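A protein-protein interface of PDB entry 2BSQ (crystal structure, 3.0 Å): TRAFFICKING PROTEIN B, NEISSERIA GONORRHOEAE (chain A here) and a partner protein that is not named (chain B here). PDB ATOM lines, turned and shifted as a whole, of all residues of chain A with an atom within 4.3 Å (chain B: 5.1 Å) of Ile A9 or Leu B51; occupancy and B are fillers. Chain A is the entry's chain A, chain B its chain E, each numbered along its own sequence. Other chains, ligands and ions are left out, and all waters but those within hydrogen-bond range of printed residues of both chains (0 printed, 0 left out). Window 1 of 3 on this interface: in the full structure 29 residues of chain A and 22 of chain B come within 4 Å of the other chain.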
ATOM      1  N   ASP A   5     -18.360  19.034 -24.815  1.00  0.00           N
ATOM      2  CA  ASP A   5     -18.617  18.339 -26.046  1.00  0.00           C
ATOM      3  C   ASP A   5     -18.531  16.857 -25.691  1.00  0.00           C
ATOM      4  O   ASP A   5     -17.825  16.472 -24.749  1.00  0.00           O
ATOM      5  CB  ASP A   5     -17.570  18.732 -27.084  1.00  0.00           C
ATOM      6  CG  ASP A   5     -18.017  18.446 -28.503  1.00  0.00           C
ATOM      7  OD1 ASP A   5     -19.173  17.997 -28.686  1.00  0.00           O
ATOM      8  OD2 ASP A   5     -17.211  18.675 -29.436  1.00  0.00           O
ATOM      9  N   THR A   6     -19.265  16.042 -26.444  1.00  0.00           N
ATOM     10  CA  THR A   6     -19.331  14.599 -26.248  1.00  0.00           C
ATOM     11  C   THR A   6     -18.058  13.922 -25.757  1.00  0.00           C
ATOM     12  O   THR A   6     -18.050  13.306 -24.690  1.00  0.00           O
ATOM     13  CB  THR A   6     -19.746  13.911 -27.540  1.00  0.00           C
ATOM     14  OG1 THR A   6     -20.890  14.579 -28.074  1.00  0.00           O
ATOM     15  CG2 THR A   6     -20.098  12.462 -27.282  1.00  0.00           C
ATOM     16  N   ASN A   7     -16.984  14.032 -26.528  1.00  0.00           N
ATOM     17  CA  ASN A   7     -15.731  13.383 -26.165  1.00  0.00           C
ATOM     18  C   ASN A   7     -15.147  13.693 -24.782  1.00  0.00           C
ATOM     19  O   ASN A   7     -14.350  12.914 -24.265  1.00  0.00           O
ATOM     20  CB  ASN A   7     -14.683  13.626 -27.256  1.00  0.00           C
ATOM     21  CG  ASN A   7     -14.267  15.067 -27.354  1.00  0.00           C
ATOM     22  OD1 ASN A   7     -13.381  15.516 -26.630  1.00  0.00           O
ATOM     23  ND2 ASN A   7     -14.915  15.813 -28.246  1.00  0.00           N
ATOM     24  N   VAL A   8     -15.518  14.803 -24.159  1.00  0.00           N
ATOM     25  CA  VAL A   8     -14.964  15.041 -22.835  1.00  0.00           C
ATOM     26  C   VAL A   8     -15.795  14.274 -21.826  1.00  0.00           C
ATOM     27  O   VAL A   8     -15.279  13.454 -21.085  1.00  0.00           O
ATOM     28  CB  VAL A   8     -14.937  16.528 -22.461  1.00  0.00           C
ATOM     29  CG1 VAL A   8     -14.419  16.679 -21.056  1.00  0.00           C
ATOM     30  CG2 VAL A   8     -14.025  17.289 -23.421  1.00  0.00           C
ATOM     31  N   ILE A   9     -17.094  14.526 -21.822  1.00  0.00           N
ATOM     32  CA  ILE A   9     -18.019  13.846 -20.923  1.00  0.00           C
ATOM     33  C   ILE A   9     -17.807  12.319 -20.993  1.00  0.00           C
ATOM     34  O   ILE A   9     -18.159  11.592 -20.072  1.00  0.00           O
ATOM     35  CB  ILE A   9     -19.480  14.201 -21.320  1.00  0.00           C
ATOM     36  CG1 ILE A   9     -20.336  14.450 -20.074  1.00  0.00           C
ATOM     37  CG2 ILE A   9     -20.071  13.092 -22.187  1.00  0.00           C
ATOM     38  CD1 ILE A   9     -20.596  13.231 -19.237  1.00  0.00           C
ATOM     39  N   SER A  10     -17.228  11.840 -22.089  1.00  0.00           N
ATOM     40  CA  SER A  10     -16.977  10.411 -22.269  1.00  0.00           C
ATOM     41  C   SER A  10     -15.680   9.954 -21.627  1.00  0.00           C
ATOM     42  O   SER A  10     -15.598   8.842 -21.101  1.00  0.00           O
ATOM     43  CB  SER A  10     -16.882  10.057 -23.752  1.00  0.00           C
ATOM     44  OG  SER A  10     -18.092  10.275 -24.435  1.00  0.00           O
ATOM     45  N   GLU A  11     -14.662  10.805 -21.681  1.00  0.00           N
ATOM     46  CA  GLU A  11     -13.359  10.440 -21.146  1.00  0.00           C
ATOM     47  C   GLU A  11     -13.317   9.694 -19.817  1.00  0.00           C
ATOM     48  O   GLU A  11     -12.671   8.656 -19.720  1.00  0.00           O
ATOM     49  CB  GLU A  11     -12.436  11.652 -21.057  1.00  0.00           C
ATOM     50  CG  GLU A  11     -10.994  11.233 -20.820  1.00  0.00           C
ATOM     51  CD  GLU A  11     -10.449  10.341 -21.942  1.00  0.00           C
ATOM     52  OE1 GLU A  11      -9.394   9.694 -21.752  1.00  0.00           O
ATOM     53  OE2 GLU A  11     -11.070  10.298 -23.024  1.00  0.00           O
ATOM     54  N   PRO A  12     -14.008  10.190 -18.781  1.00  0.00           N
ATOM     55  CA  PRO A  12     -13.971   9.490 -17.491  1.00  0.00           C
ATOM     56  C   PRO A  12     -14.565   8.081 -17.523  1.00  0.00           C
ATOM     57  O   PRO A  12     -14.099   7.179 -16.830  1.00  0.00           O
ATOM     58  CB  PRO A  12     -14.774  10.412 -16.570  1.00  0.00           C
ATOM     59  CG  PRO A  12     -14.719  11.735 -17.255  1.00  0.00           C
ATOM     60  CD  PRO A  12     -14.867  11.375 -18.698  1.00  0.00           C
ATOM     61  N   LEU A  13     -15.603   7.907 -18.331  1.00  0.00           N
ATOM     62  CA  LEU A  13     -16.301   6.637 -18.448  1.00  0.00           C
ATOM     63  C   LEU A  13     -15.474   5.571 -19.113  1.00  0.00           C
ATOM     64  O   LEU A  13     -15.819   4.395 -19.053  1.00  0.00           O
ATOM     65  CB  LEU A  13     -17.585   6.823 -19.244  1.00  0.00           C
ATOM     66  CG  LEU A  13     -18.664   7.681 -18.593  1.00  0.00           C
ATOM     67  CD1 LEU A  13     -19.777   7.914 -19.585  1.00  0.00           C
ATOM     68  CD2 LEU A  13     -19.182   6.999 -17.339  1.00  0.00           C
ATOM     69  N   MET A  43     -24.641  10.885 -26.789  1.00  0.00           N
ATOM     70  CA  MET A  43     -24.419  10.031 -25.633  1.00  0.00           C
ATOM     71  C   MET A  43     -25.485   8.953 -25.602  1.00  0.00           C
ATOM     72  O   MET A  43     -25.183   7.760 -25.541  1.00  0.00           O
ATOM     73  CB  MET A  43     -24.519  10.835 -24.346  1.00  0.00           C
ATOM     74  CG  MET A  43     -23.279  11.592 -23.946  1.00  0.00           C
ATOM     75  SD  MET A  43     -23.693  12.751 -22.593  1.00  0.00           S
ATOM     76  CE  MET A  43     -23.595  11.680 -21.127  1.00  0.00           C
ATOM     77  N   ILE A  67     -25.940  10.869 -14.268  1.00  0.00           N
ATOM     78  CA  ILE A  67     -25.315  11.873 -15.108  1.00  0.00           C
ATOM     79  C   ILE A  67     -26.297  12.969 -15.512  1.00  0.00           C
ATOM     80  O   ILE A  67     -26.469  13.943 -14.784  1.00  0.00           O
ATOM     81  CB  ILE A  67     -24.737  11.244 -16.371  1.00  0.00           C
ATOM     82  CG1 ILE A  67     -24.029   9.938 -16.016  1.00  0.00           C
ATOM     83  CG2 ILE A  67     -23.749  12.203 -17.006  1.00  0.00           C
ATOM     84  CD1 ILE A  67     -23.673   9.093 -17.214  1.00  0.00           C
ATOM     85  N   ARG B  46     -18.448  16.946  -7.827  1.00  0.00           N
ATOM     86  CA  ARG B  46     -17.251  16.954  -8.645  1.00  0.00           C
ATOM     87  C   ARG B  46     -17.511  16.079  -9.865  1.00  0.00           C
ATOM     88  O   ARG B  46     -17.367  14.860  -9.818  1.00  0.00           O
ATOM     89  CB  ARG B  46     -16.058  16.437  -7.836  1.00  0.00           C
ATOM     90  CG  ARG B  46     -15.695  17.305  -6.621  1.00  0.00           C
ATOM     91  CD  ARG B  46     -14.187  17.310  -6.367  1.00  0.00           C
ATOM     92  NE  ARG B  46     -13.640  15.953  -6.365  1.00  0.00           N
ATOM     93  CZ  ARG B  46     -12.341  15.666  -6.405  1.00  0.00           C
ATOM     94  NH1 ARG B  46     -11.452  16.654  -6.452  1.00  0.00           N
ATOM     95  NH2 ARG B  46     -11.932  14.395  -6.404  1.00  0.00           N
ATOM     96  N   LEU B  47     -17.895  16.720 -10.962  1.00  0.00           N
ATOM     97  CA  LEU B  47     -18.233  16.012 -12.184  1.00  0.00           C
ATOM     98  C   LEU B  47     -17.216  14.966 -12.625  1.00  0.00           C
ATOM     99  O   LEU B  47     -17.585  13.833 -12.933  1.00  0.00           O
ATOM    100  CB  LEU B  47     -18.477  17.018 -13.305  1.00  0.00           C
ATOM    101  CG  LEU B  47     -19.273  16.425 -14.463  1.00  0.00           C
ATOM    102  CD1 LEU B  47     -20.623  15.910 -13.954  1.00  0.00           C
ATOM    103  CD2 LEU B  47     -19.450  17.475 -15.545  1.00  0.00           C
ATOM    104  N   GLY B  48     -15.942  15.340 -12.661  1.00  0.00           N
ATOM    105  CA  GLY B  48     -14.915  14.397 -13.064  1.00  0.00           C
ATOM    106  C   GLY B  48     -14.986  13.077 -12.314  1.00  0.00           C
ATOM    107  O   GLY B  48     -15.348  12.046 -12.875  1.00  0.00           O
ATOM    108  N   SER B  49     -14.645  13.115 -11.034  1.00  0.00           N
ATOM    109  CA  SER B  49     -14.668  11.932 -10.186  1.00  0.00           C
ATOM    110  C   SER B  49     -16.008  11.215 -10.234  1.00  0.00           C
ATOM    111  O   SER B  49     -16.079   9.997 -10.077  1.00  0.00           O
ATOM    112  CB  SER B  49     -14.365  12.322  -8.745  1.00  0.00           C
ATOM    113  OG  SER B  49     -13.106  12.962  -8.652  1.00  0.00           O
ATOM    114  N   MET B  50     -17.072  11.979 -10.446  1.00  0.00           N
ATOM    115  CA  MET B  50     -18.421  11.429 -10.505  1.00  0.00           C
ATOM    116  C   MET B  50     -18.537  10.460 -11.680  1.00  0.00           C
ATOM    117  O   MET B  50     -18.873   9.287 -11.509  1.00  0.00           O
ATOM    118  CB  MET B  50     -19.422  12.573 -10.654  1.00  0.00           C
ATOM    119  CG  MET B  50     -20.682  12.419  -9.831  1.00  0.00           C
ATOM    120  SD  MET B  50     -21.664  11.019 -10.367  1.00  0.00           S
ATOM    121  CE  MET B  50     -22.217  11.614 -12.021  1.00  0.00           C
ATOM    122  N   LEU B  51     -18.243  10.963 -12.873  1.00  0.00           N
ATOM    123  CA  LEU B  51     -18.302  10.160 -14.083  1.00  0.00           C
ATOM    124  C   LEU B  51     -17.305   9.006 -14.014  1.00  0.00           C
ATOM    125  O   LEU B  51     -17.565   7.907 -14.508  1.00  0.00           O
ATOM    126  CB  LEU B  51     -18.016  11.047 -15.302  1.00  0.00           C
ATOM    127  CG  LEU B  51     -19.074  12.133 -15.531  1.00  0.00           C
ATOM    128  CD1 LEU B  51     -18.583  13.175 -16.523  1.00  0.00           C
ATOM    129  CD2 LEU B  51     -20.365  11.474 -16.006  1.00  0.00           C
ATOM    130  N   ALA B  52     -16.162   9.259 -13.392  1.00  0.00           N
ATOM    131  CA  ALA B  52     -15.137   8.237 -13.265  1.00  0.00           C
ATOM    132  C   ALA B  52     -15.703   7.035 -12.546  1.00  0.00           C
ATOM    133  O   ALA B  52     -15.548   5.905 -12.998  1.00  0.00           O
ATOM    134  CB  ALA B  52     -13.951   8.776 -12.508  1.00  0.00           C
ATOM    135  N   SER B  53     -16.356   7.277 -11.420  1.00  0.00           N
ATOM    136  CA  SER B  53     -16.939   6.188 -10.661  1.00  0.00           C
ATOM    137  C   SER B  53     -17.774   5.356 -11.606  1.00  0.00           C
ATOM    138  O   SER B  53     -17.539   4.162 -11.762  1.00  0.00           O
ATOM    139  CB  SER B  53     -17.805   6.732  -9.533  1.00  0.00           C
ATOM    140  OG  SER B  53     -17.014   7.469  -8.620  1.00  0.00           O
ATOM    141  N   ILE B  54     -18.744   6.004 -12.245  1.00  0.00           N
ATOM    142  CA  ILE B  54     -19.619   5.326 -13.195  1.00  0.00           C
ATOM    143  C   ILE B  54     -18.758   4.490 -14.125  1.00  0.00           C
ATOM    144  O   ILE B  54     -19.135   3.397 -14.520  1.00  0.00           O
ATOM    145  CB  ILE B  54     -20.399   6.314 -14.075  1.00  0.00           C
ATOM    146  CG1 ILE B  54     -21.215   7.281 -13.215  1.00  0.00           C
ATOM    147  CG2 ILE B  54     -21.293   5.538 -15.029  1.00  0.00           C
ATOM    148  CD1 ILE B  54     -22.464   6.681 -12.628  1.00  0.00           C
ATOM    149  N   GLY B  55     -17.599   5.022 -14.485  1.00  0.00           N
ATOM    150  CA  GLY B  55     -16.713   4.290 -15.363  1.00  0.00           C
ATOM    151  C   GLY B  55     -16.212   3.041 -14.675  1.00  0.00           C
ATOM    152  O   GLY B  55     -16.326   1.949 -15.219  1.00  0.00           O
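Leu B51 touches Ile A9 (CD1 to CD1, 3.4 Å). Leu B51 touches Pro A12 (CB to CB, 3.5 Å). N of Ala B52 touches CB of Pro A12, at 3.7 Å. CD2 of Leu A13 touches O of Leu B51, at 3.4 Å. Leu A13 touches Ile B54. Gly B55 touches Leu A13 (CA to O, 3.8 Å). Ile A67 touches Leu B51.
Of the printed residues of chain B, Ile A9 touches Leu B51. Glu A11 touches none of the printed residues of chain B. Of chain A, only Ile A9 (3.4 Å), Pro A12 (3.5 Å), Leu A13 (3.4 Å) and Ile A67 (3.6 Å) come within 4 Å of Leu B51. Of the printed residues of chain A, Ala B52 touches Pro A12. Of the printed residues of chain A, Ile B54 touches Leu A13. Of the printed residues of chain A, Gly B55 touches Leu A13 (3.8 Å). The nearest printed residue of chain B that does not touch Leu A13 is Ala B52 (5.1 Å).
Hydrophobic or aromatic side chains of chain B within 4 Å of the printed part of chain A: Leu B51 and Ile B54. Printed residues of chain A that touch a printed residue of chain B: Ile A9, Pro A12, Leu A13 and Ile A67. Hydrophobic or aromatic side chains of chain A within 4 Å of the printed part of chain B: Ile A9, Pro A12, Leu A13 and Ile A67. Among the printed residues, no Asp or Glu carboxylate lies within 4 Å of a Lys or Arg side-chain nitrogen of the other chain.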
